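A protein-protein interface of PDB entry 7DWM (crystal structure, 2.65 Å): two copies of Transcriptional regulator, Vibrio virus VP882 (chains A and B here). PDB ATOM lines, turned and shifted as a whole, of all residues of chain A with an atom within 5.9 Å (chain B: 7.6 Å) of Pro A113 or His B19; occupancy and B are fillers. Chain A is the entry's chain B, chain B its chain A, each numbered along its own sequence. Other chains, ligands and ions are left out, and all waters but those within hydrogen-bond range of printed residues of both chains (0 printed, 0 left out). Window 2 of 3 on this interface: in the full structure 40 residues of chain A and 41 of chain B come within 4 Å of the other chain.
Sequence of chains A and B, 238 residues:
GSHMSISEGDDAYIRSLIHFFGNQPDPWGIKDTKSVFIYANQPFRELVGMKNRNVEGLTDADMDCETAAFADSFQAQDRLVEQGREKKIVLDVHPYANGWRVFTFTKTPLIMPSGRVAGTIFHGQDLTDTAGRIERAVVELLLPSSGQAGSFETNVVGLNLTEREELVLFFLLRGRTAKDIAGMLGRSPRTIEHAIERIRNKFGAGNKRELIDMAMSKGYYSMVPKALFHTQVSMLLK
A ring nitrogen (NE2) of His B19 lies within hydrogen-bond range of the backbone carbonyl oxygen (O) of Ile A111, at 3.2 Å. N of Met A112 lies close to NE2 of His B19 (3.3 Å).
The backbone carbonyl oxygen (O) of Tyr B13 lies close to the side-chain hydroxyl (OG) of Ser B16 (3.4 Å). OD1 of Asn B23 lies close to O of His B19 (2.7 Å). The backbone carbonyl oxygen (O) of Ile A111 sits at hydrogen-bond distance from the side-chain hydroxyl (OH) of Tyr A13 (3.0 Å).
Among the printed residues, merely in contact across the chains: Tyr A13 with Ser B16 (3.7 Å), Tyr A13 with His B19 (3.4 Å), Tyr A13 with Phe B20 (3.9 Å) and Pro A113 with His B19 (3.6 Å).
Of chain B, only His B19 comes within 4 Å of Pro A113. Printed residues of chain B within 4 Å of Met A112: His B19 (3.1 Å). Of the printed residues of chain A, Ser B16 touches Tyr A13 (3.7 Å). Of the printed residues of chain A, Phe B20 touches Tyr A13 (3.9 Å). Printed residues of chain B within 4 Å of Ile A111: His B19. Printed residues of chain B within 4 Å of Tyr A13: Ser B16, His B19 and Phe B20. Ile B18 touches none of the printed residues of chain A. Leu B17 touches none of the printed residues of chain A.
Of the 8 printed residues of chain A, 4 touch a printed residue of chain B. Hydrophobic or aromatic side chains of chain A within 4 Å of the printed part of chain B: Tyr A13 and Pro A113. Hydrophobic or aromatic side chains of chain B within 4 Å of the printed part of chain A: His B19 and Phe B20.
1 position is printed for both chains. Of the 6 pairs that touch across the chains among the printed residues, none has its exchanged pair printed and touching as well.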
ATOM      1  N   GLY A   9       8.088  22.633 -26.682  1.00  0.00           N
ATOM      2  CA  GLY A   9       7.045  23.531 -27.142  1.00  0.00           C
ATOM      3  C   GLY A   9       6.629  24.565 -26.118  1.00  0.00           C
ATOM      4  O   GLY A   9       6.211  25.675 -26.480  1.00  0.00           O
ATOM      5  N   ASP A  10       6.737  24.236 -24.833  1.00  0.00           N
ATOM      6  CA  ASP A  10       6.280  25.192 -23.840  1.00  0.00           C
ATOM      7  C   ASP A  10       7.189  26.415 -23.724  1.00  0.00           C
ATOM      8  O   ASP A  10       6.695  27.492 -23.374  1.00  0.00           O
ATOM      9  CB  ASP A  10       6.100  24.496 -22.486  1.00  0.00           C
ATOM     10  CG  ASP A  10       7.368  23.830 -21.990  1.00  0.00           C
ATOM     11  OD1 ASP A  10       7.411  23.446 -20.803  1.00  0.00           O
ATOM     12  OD2 ASP A  10       8.322  23.690 -22.784  1.00  0.00           O
ATOM     13  N   TYR A  13       5.928  28.661 -26.255  1.00  0.00           N
ATOM     14  CA  TYR A  13       4.834  29.410 -25.637  1.00  0.00           C
ATOM     15  C   TYR A  13       5.367  30.533 -24.744  1.00  0.00           C
ATOM     16  O   TYR A  13       4.764  31.611 -24.667  1.00  0.00           O
ATOM     17  CB  TYR A  13       3.919  28.447 -24.871  1.00  0.00           C
ATOM     18  CG  TYR A  13       3.053  29.065 -23.778  1.00  0.00           C
ATOM     19  CD1 TYR A  13       3.558  29.270 -22.515  1.00  0.00           C
ATOM     20  CD2 TYR A  13       1.726  29.352 -23.984  1.00  0.00           C
ATOM     21  CE1 TYR A  13       2.806  29.806 -21.506  1.00  0.00           C
ATOM     22  CE2 TYR A  13       0.943  29.887 -22.964  1.00  0.00           C
ATOM     23  CZ  TYR A  13       1.493  30.104 -21.720  1.00  0.00           C
ATOM     24  OH  TYR A  13       0.725  30.636 -20.714  1.00  0.00           O
ATOM     25  N   ILE A 111       0.724  28.111 -16.500  1.00  0.00           N
ATOM     26  CA  ILE A 111       0.530  26.814 -17.136  1.00  0.00           C
ATOM     27  C   ILE A 111       0.869  26.971 -18.608  1.00  0.00           C
ATOM     28  O   ILE A 111       0.576  28.003 -19.222  1.00  0.00           O
ATOM     29  CB  ILE A 111      -0.904  26.271 -16.940  1.00  0.00           C
ATOM     30  CG1 ILE A 111      -1.281  26.294 -15.456  1.00  0.00           C
ATOM     31  CG2 ILE A 111      -1.025  24.855 -17.493  1.00  0.00           C
ATOM     32  CD1 ILE A 111      -1.018  25.003 -14.722  1.00  0.00           C
ATOM     33  N   MET A 112       1.439  25.916 -19.188  1.00  0.00           N
ATOM     34  CA  MET A 112       1.954  25.920 -20.550  1.00  0.00           C
ATOM     35  C   MET A 112       1.647  24.591 -21.241  1.00  0.00           C
ATOM     36  O   MET A 112       1.209  23.655 -20.563  1.00  0.00           O
ATOM     37  CB  MET A 112       3.449  26.206 -20.476  1.00  0.00           C
ATOM     38  CG  MET A 112       4.124  25.486 -19.362  1.00  0.00           C
ATOM     39  SD  MET A 112       5.389  26.583 -18.762  1.00  0.00           S
ATOM     40  CE  MET A 112       6.227  26.948 -20.333  1.00  0.00           C
ATOM     41  N   PRO A 113       1.888  24.434 -22.580  1.00  0.00           N
ATOM     42  CA  PRO A 113       1.396  23.224 -23.272  1.00  0.00           C
ATOM     43  C   PRO A 113       1.937  21.896 -22.761  1.00  0.00           C
ATOM     44  O   PRO A 113       1.513  20.832 -23.228  1.00  0.00           O
ATOM     45  CB  PRO A 113       1.827  23.461 -24.723  1.00  0.00           C
ATOM     46  CG  PRO A 113       1.786  24.939 -24.865  1.00  0.00           C
ATOM     47  CD  PRO A 113       2.266  25.485 -23.548  1.00  0.00           C
ATOM     48  N   SER A 114       2.878  21.931 -21.820  1.00  0.00           N
ATOM     49  CA  SER A 114       3.119  20.770 -20.968  1.00  0.00           C
ATOM     50  C   SER A 114       1.925  20.509 -20.050  1.00  0.00           C
ATOM     51  O   SER A 114       1.518  19.361 -19.854  1.00  0.00           O
ATOM     52  CB  SER A 114       4.397  20.954 -20.150  1.00  0.00           C
ATOM     53  OG  SER A 114       5.476  21.455 -20.915  1.00  0.00           O
ATOM     54  N   GLY A 115       1.346  21.569 -19.490  1.00  0.00           N
ATOM     55  CA  GLY A 115       0.366  21.436 -18.430  1.00  0.00           C
ATOM     56  C   GLY A 115       0.917  21.509 -17.020  1.00  0.00           C
ATOM     57  O   GLY A 115       0.131  21.473 -16.066  1.00  0.00           O
ATOM     58  N   TYR B  13       1.925  31.504 -32.481  1.00  0.00           N
ATOM     59  CA  TYR B  13       1.661  32.542 -31.491  1.00  0.00           C
ATOM     60  C   TYR B  13       0.179  32.605 -31.120  1.00  0.00           C
ATOM     61  O   TYR B  13      -0.168  32.783 -29.947  1.00  0.00           O
ATOM     62  CB  TYR B  13       2.175  33.881 -32.028  1.00  0.00           C
ATOM     63  CG  TYR B  13       1.764  35.104 -31.246  1.00  0.00           C
ATOM     64  CD1 TYR B  13       0.762  35.938 -31.713  1.00  0.00           C
ATOM     65  CD2 TYR B  13       2.387  35.434 -30.048  1.00  0.00           C
ATOM     66  CE1 TYR B  13       0.380  37.063 -31.009  1.00  0.00           C
ATOM     67  CE2 TYR B  13       2.009  36.564 -29.333  1.00  0.00           C
ATOM     68  CZ  TYR B  13       1.003  37.374 -29.824  1.00  0.00           C
ATOM     69  OH  TYR B  13       0.607  38.500 -29.135  1.00  0.00           O
ATOM     70  N   ILE B  14      -0.714  32.428 -32.099  1.00  0.00           N
ATOM     71  CA  ILE B  14      -2.146  32.489 -31.799  1.00  0.00           C
ATOM     72  C   ILE B  14      -2.583  31.283 -30.969  1.00  0.00           C
ATOM     73  O   ILE B  14      -3.415  31.410 -30.053  1.00  0.00           O
ATOM     74  CB  ILE B  14      -2.958  32.630 -33.103  1.00  0.00           C
ATOM     75  CG1 ILE B  14      -3.315  34.096 -33.361  1.00  0.00           C
ATOM     76  CG2 ILE B  14      -4.241  31.783 -33.072  1.00  0.00           C
ATOM     77  CD1 ILE B  14      -2.117  35.014 -33.436  1.00  0.00           C
ATOM     78  N   ARG B  15      -2.033  30.096 -31.249  1.00  0.00           N
ATOM     79  CA  ARG B  15      -2.398  28.942 -30.423  1.00  0.00           C
ATOM     80  C   ARG B  15      -1.754  29.028 -29.040  1.00  0.00           C
ATOM     81  O   ARG B  15      -2.336  28.573 -28.049  1.00  0.00           O
ATOM     82  CB  ARG B  15      -2.040  27.631 -31.115  1.00  0.00           C
ATOM     83  CG  ARG B  15      -0.571  27.227 -31.082  1.00  0.00           C
ATOM     84  CD  ARG B  15      -0.365  25.896 -31.810  1.00  0.00           C
ATOM     85  NE  ARG B  15      -0.752  25.968 -33.218  1.00  0.00           N
ATOM     86  CZ  ARG B  15      -1.906  25.525 -33.707  1.00  0.00           C
ATOM     87  NH1 ARG B  15      -2.163  25.634 -35.002  1.00  0.00           N
ATOM     88  NH2 ARG B  15      -2.807  24.981 -32.901  1.00  0.00           N
ATOM     89  N   SER B  16      -0.544  29.593 -28.964  1.00  0.00           N
ATOM     90  CA  SER B  16      -0.041  30.077 -27.685  1.00  0.00           C
ATOM     91  C   SER B  16      -1.090  30.894 -26.951  1.00  0.00           C
ATOM     92  O   SER B  16      -1.347  30.657 -25.767  1.00  0.00           O
ATOM     93  CB  SER B  16       1.233  30.889 -27.900  1.00  0.00           C
ATOM     94  OG  SER B  16       1.997  30.340 -28.969  1.00  0.00           O
ATOM     95  N   LEU B  17      -1.708  31.873 -27.612  1.00  0.00           N
ATOM     96  CA  LEU B  17      -2.519  32.809 -26.837  1.00  0.00           C
ATOM     97  C   LEU B  17      -3.877  32.221 -26.450  1.00  0.00           C
ATOM     98  O   LEU B  17      -4.429  32.590 -25.409  1.00  0.00           O
ATOM     99  CB  LEU B  17      -2.740  34.114 -27.607  1.00  0.00           C
ATOM    100  CG  LEU B  17      -1.529  34.981 -27.994  1.00  0.00           C
ATOM    101  CD1 LEU B  17      -2.040  36.224 -28.699  1.00  0.00           C
ATOM    102  CD2 LEU B  17      -0.653  35.357 -26.800  1.00  0.00           C
ATOM    103  N   ILE B  18      -4.420  31.279 -27.235  1.00  0.00           N
ATOM    104  CA  ILE B  18      -5.550  30.483 -26.727  1.00  0.00           C
ATOM    105  C   ILE B  18      -5.153  29.553 -25.583  1.00  0.00           C
ATOM    106  O   ILE B  18      -5.929  29.377 -24.633  1.00  0.00           O
ATOM    107  CB  ILE B  18      -6.388  29.757 -27.819  1.00  0.00           C
ATOM    108  CG1 ILE B  18      -6.762  30.583 -29.079  1.00  0.00           C
ATOM    109  CG2 ILE B  18      -7.310  28.689 -27.291  1.00  0.00           C
ATOM    110  CD1 ILE B  18      -6.018  30.278 -30.378  1.00  0.00           C
ATOM    111  N   HIS B  19      -3.965  28.945 -25.616  1.00  0.00           N
ATOM    112  CA  HIS B  19      -3.595  28.211 -24.407  1.00  0.00           C
ATOM    113  C   HIS B  19      -3.492  29.160 -23.212  1.00  0.00           C
ATOM    114  O   HIS B  19      -3.878  28.813 -22.090  1.00  0.00           O
ATOM    115  CB  HIS B  19      -2.290  27.442 -24.558  1.00  0.00           C
ATOM    116  CG  HIS B  19      -1.885  26.782 -23.277  1.00  0.00           C
ATOM    117  ND1 HIS B  19      -2.571  25.706 -22.753  1.00  0.00           N
ATOM    118  CD2 HIS B  19      -0.939  27.100 -22.362  1.00  0.00           C
ATOM    119  CE1 HIS B  19      -2.035  25.360 -21.597  1.00  0.00           C
ATOM    120  NE2 HIS B  19      -1.047  26.194 -21.335  1.00  0.00           N
ATOM    121  N   PHE B  20      -2.969  30.365 -23.444  1.00  0.00           N
ATOM    122  CA  PHE B  20      -2.888  31.385 -22.401  1.00  0.00           C
ATOM    123  C   PHE B  20      -4.265  31.710 -21.828  1.00  0.00           C
ATOM    124  O   PHE B  20      -4.478  31.630 -20.613  1.00  0.00           O
ATOM    125  CB  PHE B  20      -2.214  32.636 -22.976  1.00  0.00           C
ATOM    126  CG  PHE B  20      -2.218  33.818 -22.048  1.00  0.00           C
ATOM    127  CD1 PHE B  20      -2.746  35.023 -22.463  1.00  0.00           C
ATOM    128  CD2 PHE B  20      -1.664  33.739 -20.781  1.00  0.00           C
ATOM    129  CE1 PHE B  20      -2.763  36.116 -21.632  1.00  0.00           C
ATOM    130  CE2 PHE B  20      -1.663  34.840 -19.948  1.00  0.00           C
ATOM    131  CZ  PHE B  20      -2.217  36.031 -20.376  1.00  0.00           C
ATOM    132  N   PHE B  21      -5.212  32.087 -22.692  1.00  0.00           N
ATOM    133  CA  PHE B  21      -6.542  32.499 -22.247  1.00  0.00           C
ATOM    134  C   PHE B  21      -7.335  31.361 -21.612  1.00  0.00           C
ATOM    135  O   PHE B  21      -8.133  31.607 -20.701  1.00  0.00           O
ATOM    136  CB  PHE B  21      -7.329  33.087 -23.420  1.00  0.00           C
ATOM    137  CG  PHE B  21      -6.666  34.270 -24.055  1.00  0.00           C
ATOM    138  CD1 PHE B  21      -6.013  35.212 -23.281  1.00  0.00           C
ATOM    139  CD2 PHE B  21      -6.688  34.439 -25.426  1.00  0.00           C
ATOM    140  CE1 PHE B  21      -5.395  36.300 -23.867  1.00  0.00           C
ATOM    141  CE2 PHE B  21      -6.065  35.516 -26.011  1.00  0.00           C
ATOM    142  CZ  PHE B  21      -5.421  36.451 -25.232  1.00  0.00           C
ATOM    143  N   GLY B  22      -7.148  30.121 -22.072  1.00  0.00           N
ATOM    144  CA  GLY B  22      -7.918  29.014 -21.533  1.00  0.00           C
ATOM    145  C   GLY B  22      -7.646  28.646 -20.088  1.00  0.00           C
ATOM    146  O   GLY B  22      -8.303  27.736 -19.572  1.00  0.00           O
ATOM    147  N   ASN B  23      -6.710  29.312 -19.416  1.00  0.00           N
ATOM    148  CA  ASN B  23      -6.375  28.999 -18.027  1.00  0.00           C
ATOM    149  C   ASN B  23      -6.360  30.265 -17.178  1.00  0.00           C
ATOM    150  O   ASN B  23      -5.468  30.490 -16.358  1.00  0.00           O
ATOM    151  CB  ASN B  23      -5.036  28.266 -17.942  1.00  0.00           C
ATOM    152  CG  ASN B  23      -4.945  27.104 -18.908  1.00  0.00           C
ATOM    153  OD1 ASN B  23      -4.847  27.298 -20.116  1.00  0.00           O
ATOM    154  ND2 ASN B  23      -4.962  25.887 -18.379  1.00  0.00           N
ATOM    155  N   GLN B  24      -7.373  31.112 -17.367  1.00  0.00           N
ATOM    156  CA  GLN B  24      -7.646  32.255 -16.507  1.00  0.00           C
ATOM    157  C   GLN B  24      -9.139  32.305 -16.212  1.00  0.00           C
ATOM    158  O   GLN B  24      -9.957  32.098 -17.121  1.00  0.00           O
ATOM    159  CB  GLN B  24      -7.200  33.588 -17.127  1.00  0.00           C
ATOM    160  CG  GLN B  24      -5.833  33.554 -17.791  1.00  0.00           C
ATOM    161  CD  GLN B  24      -4.877  34.534 -17.157  1.00  0.00           C
ATOM    162  OE1 GLN B  24      -5.063  34.942 -16.012  1.00  0.00           O
ATOM    163  NE2 GLN B  24      -3.851  34.924 -17.894  1.00  0.00           N
ATOM    164  N   TYR B  39     -10.963  33.595 -30.922  1.00  0.00           N
ATOM    165  CA  TYR B  39     -11.127  32.693 -29.792  1.00  0.00           C
ATOM    166  C   TYR B  39     -11.653  33.469 -28.594  1.00  0.00           C
ATOM    167  O   TYR B  39     -11.449  34.680 -28.479  1.00  0.00           O
ATOM    168  CB  TYR B  39      -9.819  31.991 -29.410  1.00  0.00           C
ATOM    169  CG  TYR B  39      -9.995  31.068 -28.226  1.00  0.00           C
ATOM    170  CD1 TYR B  39      -9.510  31.417 -26.968  1.00  0.00           C
ATOM    171  CD2 TYR B  39     -10.676  29.864 -28.358  1.00  0.00           C
ATOM    172  CE1 TYR B  39      -9.694  30.582 -25.870  1.00  0.00           C
ATOM    173  CE2 TYR B  39     -10.858  29.019 -27.277  1.00  0.00           C
ATOM    174  CZ  TYR B  39     -10.362  29.378 -26.037  1.00  0.00           C
ATOM    175  OH  TYR B  39     -10.535  28.532 -24.967  1.00  0.00           O
